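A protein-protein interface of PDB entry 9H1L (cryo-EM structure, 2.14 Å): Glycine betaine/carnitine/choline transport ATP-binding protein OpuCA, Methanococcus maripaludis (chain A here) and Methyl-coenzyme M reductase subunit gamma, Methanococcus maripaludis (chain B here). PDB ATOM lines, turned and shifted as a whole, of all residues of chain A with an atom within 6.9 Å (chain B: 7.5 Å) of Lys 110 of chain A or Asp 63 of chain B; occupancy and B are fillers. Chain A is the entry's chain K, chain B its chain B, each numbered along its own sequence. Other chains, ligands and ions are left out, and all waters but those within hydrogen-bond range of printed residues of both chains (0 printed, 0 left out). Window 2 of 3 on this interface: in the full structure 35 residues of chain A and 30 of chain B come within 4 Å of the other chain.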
ATOM      1  N   ARG A  50     -37.806 -19.313 -37.786  1.00  0.00           N
ATOM      2  CA  ARG A  50     -36.844 -19.664 -36.750  1.00  0.00           C
ATOM      3  C   ARG A  50     -35.533 -20.185 -37.324  1.00  0.00           C
ATOM      4  O   ARG A  50     -34.476 -19.974 -36.719  1.00  0.00           O
ATOM      5  CB  ARG A  50     -37.466 -20.697 -35.804  1.00  0.00           C
ATOM      6  CG  ARG A  50     -36.598 -21.099 -34.627  1.00  0.00           C
ATOM      7  CD  ARG A  50     -36.415 -19.948 -33.650  1.00  0.00           C
ATOM      8  NE  ARG A  50     -35.799 -20.367 -32.396  1.00  0.00           N
ATOM      9  CZ  ARG A  50     -34.530 -20.730 -32.246  1.00  0.00           C
ATOM     10  NH1 ARG A  50     -33.670 -20.685 -33.254  1.00  0.00           N
ATOM     11  NH2 ARG A  50     -34.108 -21.131 -31.051  1.00  0.00           N
ATOM     12  N   CYS A  72     -18.822  -8.385 -29.339  1.00  0.00           N
ATOM     13  CA  CYS A  72     -19.617  -8.831 -28.201  1.00  0.00           C
ATOM     14  C   CYS A  72     -20.645  -9.871 -28.624  1.00  0.00           C
ATOM     15  O   CYS A  72     -21.172 -10.605 -27.781  1.00  0.00           O
ATOM     16  CB  CYS A  72     -20.302  -7.631 -27.550  1.00  0.00           C
ATOM     17  SG  CYS A  72     -19.270  -6.146 -27.554  1.00  0.00           S
ATOM     18  N   GLU A  73     -20.925  -9.928 -29.930  1.00  0.00           N
ATOM     19  CA  GLU A  73     -21.907 -10.833 -30.535  1.00  0.00           C
ATOM     20  C   GLU A  73     -23.298 -10.676 -29.925  1.00  0.00           C
ATOM     21  O   GLU A  73     -24.004 -11.664 -29.709  1.00  0.00           O
ATOM     22  CB  GLU A  73     -21.455 -12.296 -30.467  1.00  0.00           C
ATOM     23  CG  GLU A  73     -20.090 -12.544 -31.084  1.00  0.00           C
ATOM     24  CD  GLU A  73     -19.320 -13.643 -30.383  1.00  0.00           C
ATOM     25  OE1 GLU A  73     -19.792 -14.799 -30.395  1.00  0.00           O
ATOM     26  OE2 GLU A  73     -18.245 -13.353 -29.819  1.00  0.00           O
ATOM     27  N   ASN A  74     -23.700  -9.441 -29.646  1.00  0.00           N
ATOM     28  CA  ASN A  74     -25.055  -9.144 -29.206  1.00  0.00           C
ATOM     29  C   ASN A  74     -25.836  -8.554 -30.372  1.00  0.00           C
ATOM     30  O   ASN A  74     -25.291  -7.786 -31.172  1.00  0.00           O
ATOM     31  CB  ASN A  74     -25.034  -8.177 -28.021  1.00  0.00           C
ATOM     32  CG  ASN A  74     -26.385  -8.044 -27.355  1.00  0.00           C
ATOM     33  OD1 ASN A  74     -26.943  -6.949 -27.274  1.00  0.00           O
ATOM     34  ND2 ASN A  74     -26.922  -9.157 -26.872  1.00  0.00           N
ATOM     35  N   ILE A 104     -23.590 -13.997 -37.803  1.00  0.00           N
ATOM     36  CA  ILE A 104     -24.647 -13.353 -36.965  1.00  0.00           C
ATOM     37  C   ILE A 104     -25.822 -14.320 -36.792  1.00  0.00           C
ATOM     38  O   ILE A 104     -26.387 -14.348 -35.689  1.00  0.00           O
ATOM     39  CB  ILE A 104     -25.080 -12.021 -37.605  1.00  0.00           C
ATOM     40  CG1 ILE A 104     -24.083 -11.556 -38.670  1.00  0.00           C
ATOM     41  CG2 ILE A 104     -25.303 -10.957 -36.545  1.00  0.00           C
ATOM     42  CD1 ILE A 104     -22.832 -10.919 -38.106  1.00  0.00           C
ATOM     43  N   THR A 105     -26.181 -15.061 -37.844  1.00  0.00           N
ATOM     44  CA  THR A 105     -27.262 -16.079 -37.745  1.00  0.00           C
ATOM     45  C   THR A 105     -27.262 -16.684 -36.336  1.00  0.00           C
ATOM     46  O   THR A 105     -28.311 -16.620 -35.684  1.00  0.00           O
ATOM     47  CB  THR A 105     -27.113 -17.149 -38.833  1.00  0.00           C
ATOM     48  OG1 THR A 105     -27.600 -16.596 -40.056  1.00  0.00           O
ATOM     49  CG2 THR A 105     -27.861 -18.427 -38.524  1.00  0.00           C
ATOM     50  N   TYR A 106     -26.128 -17.236 -35.893  1.00  0.00           N
ATOM     51  CA  TYR A 106     -26.038 -17.867 -34.550  1.00  0.00           C
ATOM     52  C   TYR A 106     -26.554 -16.896 -33.483  1.00  0.00           C
ATOM     53  O   TYR A 106     -27.497 -17.254 -32.750  1.00  0.00           O
ATOM     54  CB  TYR A 106     -24.596 -18.295 -34.267  1.00  0.00           C
ATOM     55  CG  TYR A 106     -24.311 -18.680 -32.837  1.00  0.00           C
ATOM     56  CD1 TYR A 106     -25.035 -19.676 -32.203  1.00  0.00           C
ATOM     57  CD2 TYR A 106     -23.308 -18.052 -32.118  1.00  0.00           C
ATOM     58  CE1 TYR A 106     -24.776 -20.033 -30.891  1.00  0.00           C
ATOM     59  CE2 TYR A 106     -23.033 -18.400 -30.806  1.00  0.00           C
ATOM     60  CZ  TYR A 106     -23.770 -19.394 -30.190  1.00  0.00           C
ATOM     61  OH  TYR A 106     -23.503 -19.741 -28.888  1.00  0.00           O
ATOM     62  N   ALA A 107     -25.948 -15.708 -33.394  1.00  0.00           N
ATOM     63  CA  ALA A 107     -26.350 -14.720 -32.365  1.00  0.00           C
ATOM     64  C   ALA A 107     -27.822 -14.339 -32.558  1.00  0.00           C
ATOM     65  O   ALA A 107     -28.553 -14.282 -31.555  1.00  0.00           O
ATOM     66  CB  ALA A 107     -25.453 -13.511 -32.441  1.00  0.00           C
ATOM     67  N   LEU A 108     -28.233 -14.088 -33.802  1.00  0.00           N
ATOM     68  CA  LEU A 108     -29.643 -13.717 -34.094  1.00  0.00           C
ATOM     69  C   LEU A 108     -30.558 -14.866 -33.664  1.00  0.00           C
ATOM     70  O   LEU A 108     -31.589 -14.593 -33.026  1.00  0.00           O
ATOM     71  CB  LEU A 108     -29.759 -13.433 -35.594  1.00  0.00           C
ATOM     72  CG  LEU A 108     -31.173 -13.427 -36.172  1.00  0.00           C
ATOM     73  CD1 LEU A 108     -31.965 -12.237 -35.655  1.00  0.00           C
ATOM     74  CD2 LEU A 108     -31.118 -13.405 -37.690  1.00  0.00           C
ATOM     75  N   LYS A 109     -30.187 -16.102 -34.000  1.00  0.00           N
ATOM     76  CA  LYS A 109     -31.002 -17.289 -33.626  1.00  0.00           C
ATOM     77  C   LYS A 109     -31.148 -17.326 -32.101  1.00  0.00           C
ATOM     78  O   LYS A 109     -32.241 -17.678 -31.621  1.00  0.00           O
ATOM     79  CB  LYS A 109     -30.350 -18.546 -34.210  1.00  0.00           C
ATOM     80  CG  LYS A 109     -30.427 -19.810 -33.369  1.00  0.00           C
ATOM     81  CD  LYS A 109     -30.470 -21.057 -34.225  1.00  0.00           C
ATOM     82  CE  LYS A 109     -30.757 -20.759 -35.681  1.00  0.00           C
ATOM     83  NZ  LYS A 109     -32.116 -21.196 -36.079  1.00  0.00           N
ATOM     84  N   LYS A 110     -30.093 -16.953 -31.371  1.00  0.00           N
ATOM     85  CA  LYS A 110     -30.173 -16.905 -29.898  1.00  0.00           C
ATOM     86  C   LYS A 110     -31.139 -15.797 -29.497  1.00  0.00           C
ATOM     87  O   LYS A 110     -31.747 -15.886 -28.422  1.00  0.00           O
ATOM     88  CB  LYS A 110     -28.796 -16.585 -29.318  1.00  0.00           C
ATOM     89  CG  LYS A 110     -27.928 -17.779 -28.967  1.00  0.00           C
ATOM     90  CD  LYS A 110     -26.640 -17.361 -28.307  1.00  0.00           C
ATOM     91  CE  LYS A 110     -25.956 -16.231 -29.043  1.00  0.00           C
ATOM     92  NZ  LYS A 110     -24.508 -16.182 -28.745  1.00  0.00           N
ATOM     93  N   LYS A 111     -31.229 -14.761 -30.316  1.00  0.00           N
ATOM     94  CA  LYS A 111     -32.077 -13.607 -29.923  1.00  0.00           C
ATOM     95  C   LYS A 111     -33.511 -13.789 -30.391  1.00  0.00           C
ATOM     96  O   LYS A 111     -34.318 -12.865 -30.195  1.00  0.00           O
ATOM     97  CB  LYS A 111     -31.508 -12.298 -30.484  1.00  0.00           C
ATOM     98  CG  LYS A 111     -30.153 -11.886 -29.928  1.00  0.00           C
ATOM     99  CD  LYS A 111     -30.173 -11.621 -28.446  1.00  0.00           C
ATOM    100  CE  LYS A 111     -31.353 -10.771 -28.034  1.00  0.00           C
ATOM    101  NZ  LYS A 111     -31.111 -10.082 -26.747  1.00  0.00           N
ATOM    102  N   ILE A 112     -33.858 -14.971 -30.894  1.00  0.00           N
ATOM    103  CA  ILE A 112     -35.275 -15.032 -31.240  1.00  0.00           C
ATOM    104  C   ILE A 112     -35.950 -16.125 -30.425  1.00  0.00           C
ATOM    105  O   ILE A 112     -35.375 -17.193 -30.179  1.00  0.00           O
ATOM    106  CB  ILE A 112     -35.473 -15.243 -32.750  1.00  0.00           C
ATOM    107  CG1 ILE A 112     -34.801 -16.521 -33.256  1.00  0.00           C
ATOM    108  CG2 ILE A 112     -34.896 -14.048 -33.493  1.00  0.00           C
ATOM    109  CD1 ILE A 112     -34.554 -16.536 -34.769  1.00  0.00           C
ATOM    110  N   ALA A 113     -37.167 -15.845 -29.974  1.00  0.00           N
ATOM    111  CA  ALA A 113     -37.913 -16.761 -29.130  1.00  0.00           C
ATOM    112  C   ALA A 113     -38.992 -17.470 -29.935  1.00  0.00           C
ATOM    113  O   ALA A 113     -39.601 -16.891 -30.838  1.00  0.00           O
ATOM    114  CB  ALA A 113     -38.552 -16.013 -27.960  1.00  0.00           C
ATOM    115  N   TYR A 123     -37.176 -27.807 -18.479  1.00  0.00           N
ATOM    116  CA  TYR A 123     -36.236 -28.781 -17.943  1.00  0.00           C
ATOM    117  C   TYR A 123     -36.902 -29.894 -17.145  1.00  0.00           C
ATOM    118  O   TYR A 123     -36.228 -30.868 -16.796  1.00  0.00           O
ATOM    119  CB  TYR A 123     -35.188 -28.079 -17.078  1.00  0.00           C
ATOM    120  CG  TYR A 123     -34.067 -27.474 -17.887  1.00  0.00           C
ATOM    121  CD1 TYR A 123     -34.171 -26.186 -18.397  1.00  0.00           C
ATOM    122  CD2 TYR A 123     -32.912 -28.193 -18.156  1.00  0.00           C
ATOM    123  CE1 TYR A 123     -33.153 -25.629 -19.142  1.00  0.00           C
ATOM    124  CE2 TYR A 123     -31.889 -27.647 -18.903  1.00  0.00           C
ATOM    125  CZ  TYR A 123     -32.013 -26.366 -19.391  1.00  0.00           C
ATOM    126  OH  TYR A 123     -30.997 -25.816 -20.135  1.00  0.00           O
ATOM    127  N   ALA A 138     -29.673 -17.438 -17.945  1.00  0.00           N
ATOM    128  CA  ALA A 138     -29.218 -17.780 -19.313  1.00  0.00           C
ATOM    129  C   ALA A 138     -29.126 -16.504 -20.153  1.00  0.00           C
ATOM    130  O   ALA A 138     -28.024 -16.202 -20.652  1.00  0.00           O
ATOM    131  CB  ALA A 138     -30.157 -18.780 -19.939  1.00  0.00           C
ATOM    132  N   ALA A 139     -30.246 -15.792 -20.306  1.00  0.00           N
ATOM    133  CA  ALA A 139     -30.251 -14.532 -21.084  1.00  0.00           C
ATOM    134  C   ALA A 139     -29.441 -13.373 -20.498  1.00  0.00           C
ATOM    135  O   ALA A 139     -29.082 -12.458 -21.263  1.00  0.00           O
ATOM    136  CB  ALA A 139     -31.630 -13.927 -21.065  1.00  0.00           C
ATOM    137  N   LYS A 186     -36.097 -13.464 -22.277  1.00  0.00           N
ATOM    138  CA  LYS A 186     -34.820 -13.481 -22.969  1.00  0.00           C
ATOM    139  C   LYS A 186     -34.523 -12.200 -23.740  1.00  0.00           C
ATOM    140  O   LYS A 186     -33.459 -12.121 -24.363  1.00  0.00           O
ATOM    141  CB  LYS A 186     -34.745 -14.674 -23.933  1.00  0.00           C
ATOM    142  CG  LYS A 186     -36.060 -15.011 -24.600  1.00  0.00           C
ATOM    143  CD  LYS A 186     -36.017 -16.378 -25.264  1.00  0.00           C
ATOM    144  CE  LYS A 186     -35.510 -17.451 -24.317  1.00  0.00           C
ATOM    145  NZ  LYS A 186     -36.364 -17.595 -23.109  1.00  0.00           N
ATOM    146  N   ASN A 187     -35.401 -11.199 -23.677  1.00  0.00           N
ATOM    147  CA  ASN A 187     -35.346 -10.003 -24.513  1.00  0.00           C
ATOM    148  C   ASN A 187     -35.135 -10.310 -26.000  1.00  0.00           C
ATOM    149  O   ASN A 187     -34.060 -10.047 -26.546  1.00  0.00           O
ATOM    150  CB  ASN A 187     -34.276  -9.044 -24.006  1.00  0.00           C
ATOM    151  CG  ASN A 187     -34.564  -7.601 -24.371  1.00  0.00           C
ATOM    152  OD1 ASN A 187     -35.684  -7.117 -24.203  1.00  0.00           O
ATOM    153  ND2 ASN A 187     -33.551  -6.904 -24.872  1.00  0.00           N
ATOM    154  N   PRO A 188     -36.135 -10.872 -26.677  1.00  0.00           N
ATOM    155  CA  PRO A 188     -35.955 -11.239 -28.084  1.00  0.00           C
ATOM    156  C   PRO A 188     -36.040 -10.030 -29.002  1.00  0.00           C
ATOM    157  O   PRO A 188     -36.437  -8.934 -28.606  1.00  0.00           O
ATOM    158  CB  PRO A 188     -37.121 -12.200 -28.351  1.00  0.00           C
ATOM    159  CG  PRO A 188     -37.653 -12.568 -26.992  1.00  0.00           C
ATOM    160  CD  PRO A 188     -37.434 -11.344 -26.174  1.00  0.00           C
ATOM    161  N   PRO B  58     -35.715 -29.005 -26.241  1.00  0.00           N
ATOM    162  CA  PRO B  58     -35.098 -29.511 -27.472  1.00  0.00           C
ATOM    163  C   PRO B  58     -33.834 -28.743 -27.826  1.00  0.00           C
ATOM    164  O   PRO B  58     -33.656 -27.585 -27.442  1.00  0.00           O
ATOM    165  CB  PRO B  58     -36.190 -29.301 -28.527  1.00  0.00           C
ATOM    166  CG  PRO B  58     -37.452 -29.323 -27.758  1.00  0.00           C
ATOM    167  CD  PRO B  58     -37.138 -28.688 -26.439  1.00  0.00           C
ATOM    168  N   LEU B  59     -32.947 -29.417 -28.570  1.00  0.00           N
ATOM    169  CA  LEU B  59     -31.605 -28.895 -28.824  1.00  0.00           C
ATOM    170  C   LEU B  59     -31.627 -27.592 -29.613  1.00  0.00           C
ATOM    171  O   LEU B  59     -30.687 -26.796 -29.518  1.00  0.00           O
ATOM    172  CB  LEU B  59     -30.771 -29.940 -29.563  1.00  0.00           C
ATOM    173  CG  LEU B  59     -30.495 -31.250 -28.823  1.00  0.00           C
ATOM    174  CD1 LEU B  59     -29.533 -32.111 -29.616  1.00  0.00           C
ATOM    175  CD2 LEU B  59     -29.958 -30.985 -27.426  1.00  0.00           C
ATOM    176  N   GLU B  60     -32.679 -27.359 -30.400  1.00  0.00           N
ATOM    177  CA  GLU B  60     -32.826 -26.069 -31.062  1.00  0.00           C
ATOM    178  C   GLU B  60     -33.136 -24.964 -30.062  1.00  0.00           C
ATOM    179  O   GLU B  60     -32.693 -23.822 -30.230  1.00  0.00           O
ATOM    180  CB  GLU B  60     -33.911 -26.147 -32.132  1.00  0.00           C
ATOM    181  CG  GLU B  60     -33.748 -27.301 -33.102  1.00  0.00           C
ATOM    182  CD  GLU B  60     -32.872 -26.943 -34.285  1.00  0.00           C
ATOM    183  OE1 GLU B  60     -31.659 -26.714 -34.090  1.00  0.00           O
ATOM    184  OE2 GLU B  60     -33.400 -26.874 -35.413  1.00  0.00           O
ATOM    185  N   GLU B  61     -33.901 -25.281 -29.017  1.00  0.00           N
ATOM    186  CA  GLU B  61     -34.285 -24.270 -28.038  1.00  0.00           C
ATOM    187  C   GLU B  61     -33.120 -23.873 -27.140  1.00  0.00           C
ATOM    188  O   GLU B  61     -32.912 -22.683 -26.887  1.00  0.00           O
ATOM    189  CB  GLU B  61     -35.463 -24.778 -27.200  1.00  0.00           C
ATOM    190  CG  GLU B  61     -36.720 -25.258 -27.970  1.00  0.00           C
ATOM    191  CD  GLU B  61     -37.068 -24.508 -29.265  1.00  0.00           C
ATOM    192  OE1 GLU B  61     -36.874 -23.276 -29.375  1.00  0.00           O
ATOM    193  OE2 GLU B  61     -37.533 -25.180 -30.207  1.00  0.00           O
ATOM    194  N   MET B  62     -32.361 -24.849 -26.646  1.00  0.00           N
ATOM    195  CA  MET B  62     -31.204 -24.537 -25.818  1.00  0.00           C
ATOM    196  C   MET B  62     -30.091 -23.951 -26.674  1.00  0.00           C
ATOM    197  O   MET B  62     -29.885 -24.369 -27.816  1.00  0.00           O
ATOM    198  CB  MET B  62     -30.705 -25.787 -25.093  1.00  0.00           C
ATOM    199  CG  MET B  62     -31.756 -26.855 -24.887  1.00  0.00           C
ATOM    200  SD  MET B  62     -31.063 -28.359 -24.178  1.00  0.00           S
ATOM    201  CE  MET B  62     -30.166 -27.689 -22.783  1.00  0.00           C
ATOM    202  N   ASP B  63     -29.381 -22.973 -26.123  1.00  0.00           N
ATOM    203  CA  ASP B  63     -28.266 -22.335 -26.808  1.00  0.00           C
ATOM    204  C   ASP B  63     -26.963 -22.916 -26.279  1.00  0.00           C
ATOM    205  O   ASP B  63     -26.702 -22.874 -25.071  1.00  0.00           O
ATOM    206  CB  ASP B  63     -28.300 -20.818 -26.619  1.00  0.00           C
ATOM    207  CG  ASP B  63     -28.697 -20.414 -25.212  1.00  0.00           C
ATOM    208  OD1 ASP B  63     -29.838 -20.720 -24.805  1.00  0.00           O
ATOM    209  OD2 ASP B  63     -27.869 -19.794 -24.513  1.00  0.00           O
ATOM    210  N   PHE B  64     -26.154 -23.460 -27.181  1.00  0.00           N
ATOM    211  CA  PHE B  64     -24.845 -23.988 -26.846  1.00  0.00           C
ATOM    212  C   PHE B  64     -23.769 -23.104 -27.467  1.00  0.00           C
ATOM    213  O   PHE B  64     -24.044 -22.251 -28.315  1.00  0.00           O
ATOM    214  CB  PHE B  64     -24.710 -25.435 -27.325  1.00  0.00           C
ATOM    215  CG  PHE B  64     -25.773 -26.351 -26.796  1.00  0.00           C
ATOM    216  CD1 PHE B  64     -25.685 -26.870 -25.516  1.00  0.00           C
ATOM    217  CD2 PHE B  64     -26.860 -26.697 -27.580  1.00  0.00           C
ATOM    218  CE1 PHE B  64     -26.659 -27.716 -25.027  1.00  0.00           C
ATOM    219  CE2 PHE B  64     -27.840 -27.542 -27.098  1.00  0.00           C
ATOM    220  CZ  PHE B  64     -27.740 -28.052 -25.820  1.00  0.00           C
ATOM    221  N   VAL B  65     -22.530 -23.313 -27.044  1.00  0.00           N
ATOM    222  CA  VAL B  65     -21.403 -22.606 -27.628  1.00  0.00           C
ATOM    223  C   VAL B  65     -21.122 -23.188 -29.009  1.00  0.00           C
ATOM    224  O   VAL B  65     -21.557 -24.294 -29.349  1.00  0.00           O
ATOM    225  CB  VAL B  65     -20.155 -22.668 -26.726  1.00  0.00           C
ATOM    226  CG1 VAL B  65     -20.518 -22.303 -25.294  1.00  0.00           C
ATOM    227  CG2 VAL B  65     -19.520 -24.050 -26.781  1.00  0.00           C
ATOM    228  N   GLU B  66     -20.403 -22.428 -29.826  1.00  0.00           N
ATOM    229  CA  GLU B  66     -20.065 -22.878 -31.169  1.00  0.00           C
ATOM    230  C   GLU B  66     -18.932 -23.894 -31.086  1.00  0.00           C
ATOM    231  O   GLU B  66     -17.817 -23.560 -30.673  1.00  0.00           O
ATOM    232  CB  GLU B  66     -19.667 -21.693 -32.048  1.00  0.00           C
ATOM    233  CG  GLU B  66     -20.787 -21.172 -32.938  1.00  0.00           C
ATOM    234  CD  GLU B  66     -21.070 -22.073 -34.131  1.00  0.00           C
ATOM    235  OE1 GLU B  66     -20.234 -22.949 -34.438  1.00  0.00           O
ATOM    236  OE2 GLU B  66     -22.133 -21.903 -34.761  1.00  0.00           O
ATOM    237  N   ARG B  70     -18.189 -30.975 -32.035  1.00  0.00           N
ATOM    238  CA  ARG B  70     -19.398 -31.501 -31.406  1.00  0.00           C
ATOM    239  C   ARG B  70     -20.561 -31.551 -32.388  1.00  0.00           C
ATOM    240  O   ARG B  70     -21.375 -32.481 -32.348  1.00  0.00           O
ATOM    241  CB  ARG B  70     -19.763 -30.658 -30.186  1.00  0.00           C
ATOM    242  CG  ARG B  70     -20.733 -31.331 -29.233  1.00  0.00           C
ATOM    243  CD  ARG B  70     -21.554 -30.306 -28.470  1.00  0.00           C
ATOM    244  NE  ARG B  70     -21.974 -29.200 -29.321  1.00  0.00           N
ATOM    245  CZ  ARG B  70     -21.959 -27.927 -28.951  1.00  0.00           C
ATOM    246  NH1 ARG B  70     -21.548 -27.559 -27.750  1.00  0.00           N
ATOM    247  NH2 ARG B  70     -22.367 -27.000 -29.812  1.00  0.00           N
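The backbone carbonyl oxygen (O) of Glu 60 of chain B lies within hydrogen-bond range of the guanidinium group (NH2) of Arg 50 of chain A, 3.1 Å away. The guanidinium group (NH2) of Arg 50 of chain A lies within salt-bridge range of the side-chain carboxylate (OE1) of Glu 61 of chain B (3.9 Å). The backbone carbonyl oxygen (O) of Phe 64 of chain B is in hydrogen-bond range of the side-chain hydroxyl (OH) of Tyr 106 of chain A.
O of Val 65 of chain B is in hydrogen-bond range of NH2 of Arg 70 of chain B, 2.9 Å away. The backbone carbonyl oxygen of Arg 50 of chain A sits at hydrogen-bond distance from the side-chain amino group of Lys 109 of chain A, 2.7 Å away.
Val 65 of chain B touches Tyr 106 of chain A (CA to OH, 3.8 Å). Lys 110 of chain A touches Asp 63 of chain B (CG to CB, 3.9 Å). Tyr 123 of chain A touches Met 62 of chain B (OH to CE, 3.3 Å).
Of the printed residues of chain B, Arg 50 of chain A touches Glu 60 and Glu 61. Glu 73 of chain A touches none of the printed residues of chain B. Of chain B, only Asp 63 comes within 4 Å of Lys 110 of chain A. Printed residues of chain B within 4 Å of Tyr 123 of chain A: Met 62 (3.3 Å). Asn 187 of chain A touches none of the printed residues of chain B. Of the printed residues of chain A, Glu 60 of chain B touches Arg 50 (3.1 Å). Printed residues of chain A within 4 Å of Glu 61 of chain B: Arg 50 (3.9 Å). Asp 63 of chain B touches just one residue of chain A: Lys 110. Of the printed residues of chain A, Val 65 of chain B touches Tyr 106.
Of the 10 printed residues of chain B, 6 touch a printed residue of chain A. Along chain B the printed residues that touch a printed residue of chain A span positions 60 to 65. Printed residues of chain A that touch a printed residue of chain B: Arg 50, Tyr 106, Lys 110 and Tyr 123. Hydrophobic or aromatic side chains of chain A that line the printed part of chain B: Tyr 106 and Tyr 123.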
